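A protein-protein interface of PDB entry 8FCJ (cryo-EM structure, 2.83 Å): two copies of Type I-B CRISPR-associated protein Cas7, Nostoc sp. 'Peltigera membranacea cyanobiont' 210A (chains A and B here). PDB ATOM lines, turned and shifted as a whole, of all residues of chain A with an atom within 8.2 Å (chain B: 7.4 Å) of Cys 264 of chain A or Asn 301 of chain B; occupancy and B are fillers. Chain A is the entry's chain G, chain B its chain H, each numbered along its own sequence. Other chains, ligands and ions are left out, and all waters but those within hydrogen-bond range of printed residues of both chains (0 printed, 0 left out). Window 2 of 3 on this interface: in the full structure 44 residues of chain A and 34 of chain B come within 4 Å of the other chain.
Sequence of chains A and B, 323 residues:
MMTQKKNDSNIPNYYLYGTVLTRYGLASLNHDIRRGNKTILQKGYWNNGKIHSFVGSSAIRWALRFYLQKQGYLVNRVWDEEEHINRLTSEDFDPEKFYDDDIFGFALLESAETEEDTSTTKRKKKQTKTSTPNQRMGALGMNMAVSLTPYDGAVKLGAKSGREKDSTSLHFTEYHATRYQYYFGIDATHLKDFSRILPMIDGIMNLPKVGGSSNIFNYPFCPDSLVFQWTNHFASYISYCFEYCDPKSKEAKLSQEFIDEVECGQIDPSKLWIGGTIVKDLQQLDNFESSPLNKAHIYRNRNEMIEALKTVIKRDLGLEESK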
ATOM      1  N   TYR A 237     -26.402   6.548 -38.940  1.00  0.00           N
ATOM      2  CA  TYR A 237     -25.368   7.523 -38.622  1.00  0.00           C
ATOM      3  C   TYR A 237     -24.077   7.237 -39.379  1.00  0.00           C
ATOM      4  O   TYR A 237     -22.983   7.503 -38.877  1.00  0.00           O
ATOM      5  CB  TYR A 237     -25.107   7.558 -37.118  1.00  0.00           C
ATOM      6  CG  TYR A 237     -26.281   8.051 -36.314  1.00  0.00           C
ATOM      7  CD1 TYR A 237     -26.496   9.407 -36.130  1.00  0.00           C
ATOM      8  CD2 TYR A 237     -27.178   7.162 -35.745  1.00  0.00           C
ATOM      9  CE1 TYR A 237     -27.567   9.863 -35.401  1.00  0.00           C
ATOM     10  CE2 TYR A 237     -28.255   7.610 -35.012  1.00  0.00           C
ATOM     11  CZ  TYR A 237     -28.444   8.962 -34.844  1.00  0.00           C
ATOM     12  OH  TYR A 237     -29.516   9.417 -34.114  1.00  0.00           O
ATOM     13  N   GLU A 257     -15.978  11.684 -36.244  1.00  0.00           N
ATOM     14  CA  GLU A 257     -17.336  11.665 -35.706  1.00  0.00           C
ATOM     15  C   GLU A 257     -17.914  10.256 -35.717  1.00  0.00           C
ATOM     16  O   GLU A 257     -18.554   9.832 -34.749  1.00  0.00           O
ATOM     17  CB  GLU A 257     -18.243  12.618 -36.489  1.00  0.00           C
ATOM     18  CG  GLU A 257     -17.807  14.096 -36.595  1.00  0.00           C
ATOM     19  CD  GLU A 257     -16.517  14.349 -37.373  1.00  0.00           C
ATOM     20  OE1 GLU A 257     -16.343  15.490 -37.850  1.00  0.00           O
ATOM     21  OE2 GLU A 257     -15.683  13.433 -37.524  1.00  0.00           O
ATOM     22  N   PHE A 258     -17.702   9.516 -36.807  1.00  0.00           N
ATOM     23  CA  PHE A 258     -18.192   8.144 -36.880  1.00  0.00           C
ATOM     24  C   PHE A 258     -17.532   7.270 -35.822  1.00  0.00           C
ATOM     25  O   PHE A 258     -18.204   6.476 -35.148  1.00  0.00           O
ATOM     26  CB  PHE A 258     -17.944   7.588 -38.281  1.00  0.00           C
ATOM     27  CG  PHE A 258     -18.239   6.126 -38.416  1.00  0.00           C
ATOM     28  CD1 PHE A 258     -19.537   5.679 -38.563  1.00  0.00           C
ATOM     29  CD2 PHE A 258     -17.214   5.198 -38.411  1.00  0.00           C
ATOM     30  CE1 PHE A 258     -19.809   4.337 -38.694  1.00  0.00           C
ATOM     31  CE2 PHE A 258     -17.482   3.854 -38.540  1.00  0.00           C
ATOM     32  CZ  PHE A 258     -18.781   3.424 -38.681  1.00  0.00           C
ATOM     33  N   ILE A 259     -16.217   7.415 -35.649  1.00  0.00           N
ATOM     34  CA  ILE A 259     -15.512   6.643 -34.633  1.00  0.00           C
ATOM     35  C   ILE A 259     -16.034   6.990 -33.247  1.00  0.00           C
ATOM     36  O   ILE A 259     -16.253   6.105 -32.414  1.00  0.00           O
ATOM     37  CB  ILE A 259     -13.995   6.877 -34.745  1.00  0.00           C
ATOM     38  CG1 ILE A 259     -13.457   6.245 -36.028  1.00  0.00           C
ATOM     39  CG2 ILE A 259     -13.276   6.311 -33.535  1.00  0.00           C
ATOM     40  CD1 ILE A 259     -11.959   6.334 -36.167  1.00  0.00           C
ATOM     41  N   ASP A 260     -16.252   8.279 -32.981  1.00  0.00           N
ATOM     42  CA  ASP A 260     -16.764   8.694 -31.680  1.00  0.00           C
ATOM     43  C   ASP A 260     -18.154   8.129 -31.426  1.00  0.00           C
ATOM     44  O   ASP A 260     -18.467   7.708 -30.307  1.00  0.00           O
ATOM     45  CB  ASP A 260     -16.784  10.219 -31.587  1.00  0.00           C
ATOM     46  CG  ASP A 260     -15.481  10.788 -31.073  1.00  0.00           C
ATOM     47  OD1 ASP A 260     -14.751  10.061 -30.366  1.00  0.00           O
ATOM     48  OD2 ASP A 260     -15.185  11.962 -31.374  1.00  0.00           O
ATOM     49  N   GLU A 261     -19.006   8.122 -32.451  1.00  0.00           N
ATOM     50  CA  GLU A 261     -20.348   7.578 -32.286  1.00  0.00           C
ATOM     51  C   GLU A 261     -20.320   6.072 -32.080  1.00  0.00           C
ATOM     52  O   GLU A 261     -21.213   5.522 -31.428  1.00  0.00           O
ATOM     53  CB  GLU A 261     -21.214   7.943 -33.488  1.00  0.00           C
ATOM     54  CG  GLU A 261     -21.594   9.410 -33.524  1.00  0.00           C
ATOM     55  CD  GLU A 261     -22.734   9.696 -34.471  1.00  0.00           C
ATOM     56  OE1 GLU A 261     -22.749   9.110 -35.573  1.00  0.00           O
ATOM     57  OE2 GLU A 261     -23.614  10.506 -34.116  1.00  0.00           O
ATOM     58  N   VAL A 262     -19.320   5.386 -32.634  1.00  0.00           N
ATOM     59  CA  VAL A 262     -19.157   3.970 -32.315  1.00  0.00           C
ATOM     60  C   VAL A 262     -18.684   3.797 -30.874  1.00  0.00           C
ATOM     61  O   VAL A 262     -19.157   2.909 -30.155  1.00  0.00           O
ATOM     62  CB  VAL A 262     -18.197   3.298 -33.311  1.00  0.00           C
ATOM     63  CG1 VAL A 262     -17.955   1.856 -32.912  1.00  0.00           C
ATOM     64  CG2 VAL A 262     -18.767   3.361 -34.712  1.00  0.00           C
ATOM     65  N   GLU A 263     -17.746   4.640 -30.432  1.00  0.00           N
ATOM     66  CA  GLU A 263     -17.219   4.527 -29.074  1.00  0.00           C
ATOM     67  C   GLU A 263     -18.301   4.769 -28.030  1.00  0.00           C
ATOM     68  O   GLU A 263     -18.381   4.049 -27.029  1.00  0.00           O
ATOM     69  CB  GLU A 263     -16.066   5.510 -28.861  1.00  0.00           C
ATOM     70  CG  GLU A 263     -14.915   5.387 -29.841  1.00  0.00           C
ATOM     71  CD  GLU A 263     -13.798   4.503 -29.334  1.00  0.00           C
ATOM     72  OE1 GLU A 263     -14.095   3.445 -28.750  1.00  0.00           O
ATOM     73  OE2 GLU A 263     -12.619   4.868 -29.524  1.00  0.00           O
ATOM     74  N   CYS A 264     -19.141   5.784 -28.243  1.00  0.00           N
ATOM     75  CA  CYS A 264     -20.134   6.147 -27.239  1.00  0.00           C
ATOM     76  C   CYS A 264     -21.259   5.127 -27.131  1.00  0.00           C
ATOM     77  O   CYS A 264     -22.052   5.199 -26.188  1.00  0.00           O
ATOM     78  CB  CYS A 264     -20.713   7.527 -27.544  1.00  0.00           C
ATOM     79  SG  CYS A 264     -21.877   7.564 -28.919  1.00  0.00           S
ATOM     80  N   GLY A 265     -21.348   4.187 -28.063  1.00  0.00           N
ATOM     81  CA  GLY A 265     -22.392   3.188 -28.043  1.00  0.00           C
ATOM     82  C   GLY A 265     -23.624   3.523 -28.850  1.00  0.00           C
ATOM     83  O   GLY A 265     -24.589   2.751 -28.817  1.00  0.00           O
ATOM     84  N   GLN A 266     -23.630   4.650 -29.565  1.00  0.00           N
ATOM     85  CA  GLN A 266     -24.788   5.001 -30.379  1.00  0.00           C
ATOM     86  C   GLN A 266     -25.023   3.977 -31.479  1.00  0.00           C
ATOM     87  O   GLN A 266     -26.162   3.555 -31.712  1.00  0.00           O
ATOM     88  CB  GLN A 266     -24.604   6.392 -30.979  1.00  0.00           C
ATOM     89  CG  GLN A 266     -25.642   6.742 -32.020  1.00  0.00           C
ATOM     90  CD  GLN A 266     -26.996   7.018 -31.412  1.00  0.00           C
ATOM     91  OE1 GLN A 266     -27.196   8.039 -30.761  1.00  0.00           O
ATOM     92  NE2 GLN A 266     -27.934   6.105 -31.616  1.00  0.00           N
ATOM     93  N   ILE A 267     -23.963   3.565 -32.163  1.00  0.00           N
ATOM     94  CA  ILE A 267     -24.051   2.588 -33.242  1.00  0.00           C
ATOM     95  C   ILE A 267     -23.744   1.218 -32.660  1.00  0.00           C
ATOM     96  O   ILE A 267     -22.691   1.017 -32.046  1.00  0.00           O
ATOM     97  CB  ILE A 267     -23.091   2.930 -34.389  1.00  0.00           C
ATOM     98  CG1 ILE A 267     -23.438   4.294 -34.985  1.00  0.00           C
ATOM     99  CG2 ILE A 267     -23.145   1.858 -35.458  1.00  0.00           C
ATOM    100  CD1 ILE A 267     -22.579   4.676 -36.165  1.00  0.00           C
ATOM    101  N   SER A 291     -11.482  -1.124 -28.112  1.00  0.00           N
ATOM    102  CA  SER A 291     -12.550  -0.268 -28.596  1.00  0.00           C
ATOM    103  C   SER A 291     -13.786  -1.090 -28.959  1.00  0.00           C
ATOM    104  O   SER A 291     -13.672  -2.246 -29.372  1.00  0.00           O
ATOM    105  CB  SER A 291     -12.086   0.520 -29.815  1.00  0.00           C
ATOM    106  OG  SER A 291     -13.189   1.015 -30.551  1.00  0.00           O
ATOM    107  N   PRO A 292     -14.979  -0.512 -28.805  1.00  0.00           N
ATOM    108  CA  PRO A 292     -16.189  -1.191 -29.294  1.00  0.00           C
ATOM    109  C   PRO A 292     -16.195  -1.399 -30.795  1.00  0.00           C
ATOM    110  O   PRO A 292     -16.960  -2.236 -31.285  1.00  0.00           O
ATOM    111  CB  PRO A 292     -17.320  -0.251 -28.855  1.00  0.00           C
ATOM    112  CG  PRO A 292     -16.757   0.498 -27.702  1.00  0.00           C
ATOM    113  CD  PRO A 292     -15.300   0.677 -28.000  1.00  0.00           C
ATOM    114  N   LEU A 293     -15.380  -0.655 -31.542  1.00  0.00           N
ATOM    115  CA  LEU A 293     -15.264  -0.886 -32.975  1.00  0.00           C
ATOM    116  C   LEU A 293     -14.690  -2.261 -33.287  1.00  0.00           C
ATOM    117  O   LEU A 293     -14.892  -2.769 -34.395  1.00  0.00           O
ATOM    118  CB  LEU A 293     -14.396   0.202 -33.606  1.00  0.00           C
ATOM    119  CG  LEU A 293     -14.410   0.337 -35.128  1.00  0.00           C
ATOM    120  CD1 LEU A 293     -15.744   0.867 -35.614  1.00  0.00           C
ATOM    121  CD2 LEU A 293     -13.282   1.244 -35.577  1.00  0.00           C
ATOM    122  N   MET B 205     -36.809  10.296 -32.854  1.00  0.00           N
ATOM    123  CA  MET B 205     -35.424   9.867 -33.020  1.00  0.00           C
ATOM    124  C   MET B 205     -35.255   8.963 -34.235  1.00  0.00           C
ATOM    125  O   MET B 205     -34.304   9.127 -35.006  1.00  0.00           O
ATOM    126  CB  MET B 205     -34.918   9.178 -31.757  1.00  0.00           C
ATOM    127  CG  MET B 205     -35.435   9.791 -30.484  1.00  0.00           C
ATOM    128  SD  MET B 205     -34.318  11.092 -29.951  1.00  0.00           S
ATOM    129  CE  MET B 205     -32.744  10.251 -30.084  1.00  0.00           C
ATOM    130  N   ILE B 274     -29.628  17.393 -23.082  1.00  0.00           N
ATOM    131  CA  ILE B 274     -28.766  17.674 -24.222  1.00  0.00           C
ATOM    132  C   ILE B 274     -28.049  16.392 -24.611  1.00  0.00           C
ATOM    133  O   ILE B 274     -27.462  15.720 -23.756  1.00  0.00           O
ATOM    134  CB  ILE B 274     -27.752  18.788 -23.904  1.00  0.00           C
ATOM    135  CG1 ILE B 274     -28.479  20.049 -23.443  1.00  0.00           C
ATOM    136  CG2 ILE B 274     -26.893  19.085 -25.114  1.00  0.00           C
ATOM    137  CD1 ILE B 274     -27.553  21.181 -23.079  1.00  0.00           C
ATOM    138  N   GLY B 275     -28.100  16.051 -25.898  1.00  0.00           N
ATOM    139  CA  GLY B 275     -27.438  14.860 -26.385  1.00  0.00           C
ATOM    140  C   GLY B 275     -27.030  15.012 -27.832  1.00  0.00           C
ATOM    141  O   GLY B 275     -27.438  15.947 -28.523  1.00  0.00           O
ATOM    142  N   GLY B 276     -26.213  14.074 -28.283  1.00  0.00           N
ATOM    143  CA  GLY B 276     -25.714  14.067 -29.637  1.00  0.00           C
ATOM    144  C   GLY B 276     -24.276  14.534 -29.726  1.00  0.00           C
ATOM    145  O   GLY B 276     -23.518  14.519 -28.754  1.00  0.00           O
ATOM    146  N   THR B 277     -23.899  14.965 -30.930  1.00  0.00           N
ATOM    147  CA  THR B 277     -22.527  15.389 -31.174  1.00  0.00           C
ATOM    148  C   THR B 277     -22.214  16.751 -30.572  1.00  0.00           C
ATOM    149  O   THR B 277     -21.036  17.104 -30.459  1.00  0.00           O
ATOM    150  CB  THR B 277     -22.242  15.419 -32.676  1.00  0.00           C
ATOM    151  OG1 THR B 277     -20.858  15.716 -32.892  1.00  0.00           O
ATOM    152  CG2 THR B 277     -23.081  16.483 -33.350  1.00  0.00           C
ATOM    153  N   VAL B 279     -22.557  17.449 -27.573  1.00  0.00           N
ATOM    154  CA  VAL B 279     -22.045  17.197 -26.230  1.00  0.00           C
ATOM    155  C   VAL B 279     -20.529  17.332 -26.203  1.00  0.00           C
ATOM    156  O   VAL B 279     -19.954  17.866 -25.247  1.00  0.00           O
ATOM    157  CB  VAL B 279     -22.504  15.811 -25.745  1.00  0.00           C
ATOM    158  CG1 VAL B 279     -21.670  15.346 -24.569  1.00  0.00           C
ATOM    159  CG2 VAL B 279     -23.974  15.846 -25.383  1.00  0.00           C
ATOM    160  N   ILE B 298     -26.732  15.677 -19.608  1.00  0.00           N
ATOM    161  CA  ILE B 298     -25.928  15.698 -20.823  1.00  0.00           C
ATOM    162  C   ILE B 298     -25.399  14.294 -21.072  1.00  0.00           C
ATOM    163  O   ILE B 298     -24.691  13.733 -20.228  1.00  0.00           O
ATOM    164  CB  ILE B 298     -24.778  16.710 -20.718  1.00  0.00           C
ATOM    165  CG1 ILE B 298     -25.327  18.134 -20.773  1.00  0.00           C
ATOM    166  CG2 ILE B 298     -23.768  16.484 -21.819  1.00  0.00           C
ATOM    167  CD1 ILE B 298     -24.268  19.194 -20.682  1.00  0.00           C
ATOM    168  N   TYR B 299     -25.741  13.731 -22.228  1.00  0.00           N
ATOM    169  CA  TYR B 299     -25.300  12.401 -22.623  1.00  0.00           C
ATOM    170  C   TYR B 299     -24.800  12.452 -24.056  1.00  0.00           C
ATOM    171  O   TYR B 299     -25.501  12.954 -24.938  1.00  0.00           O
ATOM    172  CB  TYR B 299     -26.437  11.379 -22.516  1.00  0.00           C
ATOM    173  CG  TYR B 299     -27.035  11.233 -21.139  1.00  0.00           C
ATOM    174  CD1 TYR B 299     -28.014  12.105 -20.689  1.00  0.00           C
ATOM    175  CD2 TYR B 299     -26.633  10.210 -20.294  1.00  0.00           C
ATOM    176  CE1 TYR B 299     -28.567  11.970 -19.436  1.00  0.00           C
ATOM    177  CE2 TYR B 299     -27.181  10.068 -19.038  1.00  0.00           C
ATOM    178  CZ  TYR B 299     -28.147  10.951 -18.615  1.00  0.00           C
ATOM    179  OH  TYR B 299     -28.696  10.812 -17.362  1.00  0.00           O
ATOM    180  N   ARG B 300     -23.594  11.933 -24.292  1.00  0.00           N
ATOM    181  CA  ARG B 300     -23.120  11.809 -25.665  1.00  0.00           C
ATOM    182  C   ARG B 300     -23.983  10.830 -26.450  1.00  0.00           C
ATOM    183  O   ARG B 300     -24.323  11.079 -27.611  1.00  0.00           O
ATOM    184  CB  ARG B 300     -21.655  11.374 -25.685  1.00  0.00           C
ATOM    185  CG  ARG B 300     -20.798  12.126 -26.695  1.00  0.00           C
ATOM    186  CD  ARG B 300     -21.328  11.953 -28.106  1.00  0.00           C
ATOM    187  NE  ARG B 300     -20.345  12.299 -29.124  1.00  0.00           N
ATOM    188  CZ  ARG B 300     -20.512  12.090 -30.421  1.00  0.00           C
ATOM    189  NH1 ARG B 300     -21.614  11.533 -30.895  1.00  0.00           N
ATOM    190  NH2 ARG B 300     -19.550  12.450 -31.266  1.00  0.00           N
ATOM    191  N   ASN B 301     -24.354   9.715 -25.829  1.00  0.00           N
ATOM    192  CA  ASN B 301     -25.200   8.725 -26.479  1.00  0.00           C
ATOM    193  C   ASN B 301     -26.646   9.200 -26.444  1.00  0.00           C
ATOM    194  O   ASN B 301     -27.193   9.462 -25.368  1.00  0.00           O
ATOM    195  CB  ASN B 301     -25.055   7.374 -25.785  1.00  0.00           C
ATOM    196  CG  ASN B 301     -25.668   6.242 -26.578  1.00  0.00           C
ATOM    197  OD1 ASN B 301     -26.360   6.464 -27.569  1.00  0.00           O
ATOM    198  ND2 ASN B 301     -25.413   5.014 -26.146  1.00  0.00           N
ATOM    199  N   ARG B 302     -27.266   9.315 -27.620  1.00  0.00           N
ATOM    200  CA  ARG B 302     -28.660   9.736 -27.674  1.00  0.00           C
ATOM    201  C   ARG B 302     -29.583   8.692 -27.065  1.00  0.00           C
ATOM    202  O   ARG B 302     -30.593   9.046 -26.446  1.00  0.00           O
ATOM    203  CB  ARG B 302     -29.072  10.025 -29.115  1.00  0.00           C
ATOM    204  CG  ARG B 302     -28.284  11.137 -29.774  1.00  0.00           C
ATOM    205  CD  ARG B 302     -28.363  11.032 -31.282  1.00  0.00           C
ATOM    206  NE  ARG B 302     -27.246  11.701 -31.936  1.00  0.00           N
ATOM    207  CZ  ARG B 302     -26.037  11.178 -32.075  1.00  0.00           C
ATOM    208  NH1 ARG B 302     -25.744   9.980 -31.600  1.00  0.00           N
ATOM    209  NH2 ARG B 302     -25.097  11.875 -32.706  1.00  0.00           N
ATOM    210  N   ASN B 303     -29.262   7.408 -27.231  1.00  0.00           N
ATOM    211  CA  ASN B 303     -30.095   6.356 -26.659  1.00  0.00           C
ATOM    212  C   ASN B 303     -30.119   6.432 -25.139  1.00  0.00           C
ATOM    213  O   ASN B 303     -31.175   6.271 -24.521  1.00  0.00           O
ATOM    214  CB  ASN B 303     -29.600   4.988 -27.120  1.00  0.00           C
ATOM    215  CG  ASN B 303     -29.704   4.808 -28.617  1.00  0.00           C
ATOM    216  OD1 ASN B 303     -30.172   5.694 -29.328  1.00  0.00           O
ATOM    217  ND2 ASN B 303     -29.265   3.655 -29.105  1.00  0.00           N
ATOM    218  N   GLU B 304     -28.962   6.672 -24.517  1.00  0.00           N
ATOM    219  CA  GLU B 304     -28.916   6.778 -23.062  1.00  0.00           C
ATOM    220  C   GLU B 304     -29.731   7.965 -22.567  1.00  0.00           C
ATOM    221  O   GLU B 304     -30.484   7.851 -21.590  1.00  0.00           O
ATOM    222  CB  GLU B 304     -27.469   6.893 -22.590  1.00  0.00           C
ATOM    223  CG  GLU B 304     -26.678   5.606 -22.688  1.00  0.00           C
ATOM    224  CD  GLU B 304     -25.297   5.730 -22.080  1.00  0.00           C
ATOM    225  OE1 GLU B 304     -25.044   6.730 -21.377  1.00  0.00           O
ATOM    226  OE2 GLU B 304     -24.464   4.827 -22.306  1.00  0.00           O
ATOM    227  N   MET B 305     -29.591   9.117 -23.228  1.00  0.00           N
ATOM    228  CA  MET B 305     -30.347  10.291 -22.811  1.00  0.00           C
ATOM    229  C   MET B 305     -31.839  10.060 -22.983  1.00  0.00           C
ATOM    230  O   MET B 305     -32.638  10.465 -22.134  1.00  0.00           O
ATOM    231  CB  MET B 305     -29.920  11.523 -23.601  1.00  0.00           C
ATOM    232  CG  MET B 305     -30.678  12.770 -23.180  1.00  0.00           C
ATOM    233  SD  MET B 305     -31.787  13.412 -24.440  1.00  0.00           S
ATOM    234  CE  MET B 305     -30.636  13.666 -25.772  1.00  0.00           C
ATOM    235  N   ILE B 306     -32.233   9.416 -24.080  1.00  0.00           N
ATOM    236  CA  ILE B 306     -33.647   9.152 -24.314  1.00  0.00           C
ATOM    237  C   ILE B 306     -34.187   8.174 -23.280  1.00  0.00           C
ATOM    238  O   ILE B 306     -35.314   8.321 -22.804  1.00  0.00           O
ATOM    239  CB  ILE B 306     -33.864   8.653 -25.751  1.00  0.00           C
ATOM    240  CG1 ILE B 306     -33.779   9.829 -26.717  1.00  0.00           C
ATOM    241  CG2 ILE B 306     -35.208   7.972 -25.892  1.00  0.00           C
ATOM    242  CD1 ILE B 306     -34.686  10.977 -26.352  1.00  0.00           C
ATOM    243  N   GLU B 307     -33.394   7.167 -22.909  1.00  0.00           N
ATOM    244  CA  GLU B 307     -33.831   6.237 -21.873  1.00  0.00           C
ATOM    245  C   GLU B 307     -34.022   6.946 -20.539  1.00  0.00           C
ATOM    246  O   GLU B 307     -35.028   6.731 -19.851  1.00  0.00           O
ATOM    247  CB  GLU B 307     -32.829   5.095 -21.735  1.00  0.00           C
ATOM    248  CG  GLU B 307     -32.930   4.055 -22.835  1.00  0.00           C
ATOM    249  CD  GLU B 307     -34.357   3.619 -23.089  1.00  0.00           C
ATOM    250  OE1 GLU B 307     -35.031   3.190 -22.129  1.00  0.00           O
ATOM    251  OE2 GLU B 307     -34.810   3.706 -24.250  1.00  0.00           O
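The side-chain carboxylate (OE2) of Glu 261 of chain A lies within salt-bridge range of the guanidinium group (NH1) of Arg 300 of chain B (3.9 Å).
The guanidinium group (NH2) of Arg 302 of chain B lies within salt-bridge range of the side-chain carboxylate (OE2) of Glu 261 of chain A (2.5 Å).
The side-chain amide nitrogen (ND2) of Asn 301 of chain B is in hydrogen-bond range of the backbone carbonyl oxygen (O) of Cys 264 of chain A, at 3.4 Å.
OD1 of Asn 303 of chain B lies within hydrogen-bond range of NE2 of Gln 266 of chain A, at 3.2 Å.
The guanidinium group (NH1) of Arg 302 of chain B is in hydrogen-bond range of the side-chain amide oxygen (OE1) of Gln 266 of chain A, at 2.6 Å.
N of Ile 267 of chain A sits at hydrogen-bond distance from O of Glu 261 of chain A, 3.5 Å away.
The side-chain sulfur of Cys 264 of chain A sits close to the backbone NH of Gln 266 of chain A, 3.5 Å away.
The backbone NH (N) of Gln 266 of chain A lies within hydrogen-bond range of the backbone carbonyl oxygen (O) of Glu 261 of chain A.
OD1 of Asn 301 of chain B lies within hydrogen-bond range of N of Asn 303 of chain B, 3.1 Å away.
SG of Cys 264 of chain A lies within hydrogen-bond range of O of Glu 261 of chain A, at 3.3 Å.
The backbone carbonyl oxygen of Asp 260 of chain A sits close to the side-chain sulfur of Cys 264 of chain A, 3.7 Å away.
Among the printed residues, pairs that only touch across the chains: Tyr 237 of chain A with Arg 302 of chain B (3.5 Å), Asp 260 of chain A with Arg 300 of chain B (3.6 Å), Gly 265 of chain A with Asn 301 of chain B (3.6 Å) and Gln 266 of chain A with Asn 301 of chain B (3.5 Å).
Of chain B, only Asn 301 comes within 4 Å of Cys 264 of chain A.
Printed residues of chain A within 4 Å of Asn 301 of chain B: Cys 264 (3.4 Å), Gly 265 (3.6 Å) and Gln 266 (3.5 Å).
Printed residues of chain B within 4 Å of Tyr 237 of chain A: Arg 302.
Of the printed residues of chain B, Gly 265 of chain A touches Asn 301 (3.6 Å).
Ile 298 of chain B touches none of the printed residues of chain A.
The nearest residue of chain B that does not touch Cys 264 of chain A is Arg 300 of chain B (4.4 Å).
The nearest printed residue of chain B that does not touch Glu 261 of chain A is Thr 277 of chain B (5.3 Å).
Printed residues of chain A that touch a printed residue of chain B: Tyr 237, Asp 260, Glu 261, Cys 264, Gly 265 and Gln 266.
Among the printed residues, 9 pairs touch across the chains.
Among the printed residues, Asp or Glu carboxylates within 4 Å of a Lys or Arg side-chain nitrogen of the other chain: Glu 261 of chain A with Arg 300 of chain B (3.9 Å) and Glu 261 of chain A with Arg 302 of chain B (2.5 Å).
No position is printed for both chains.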
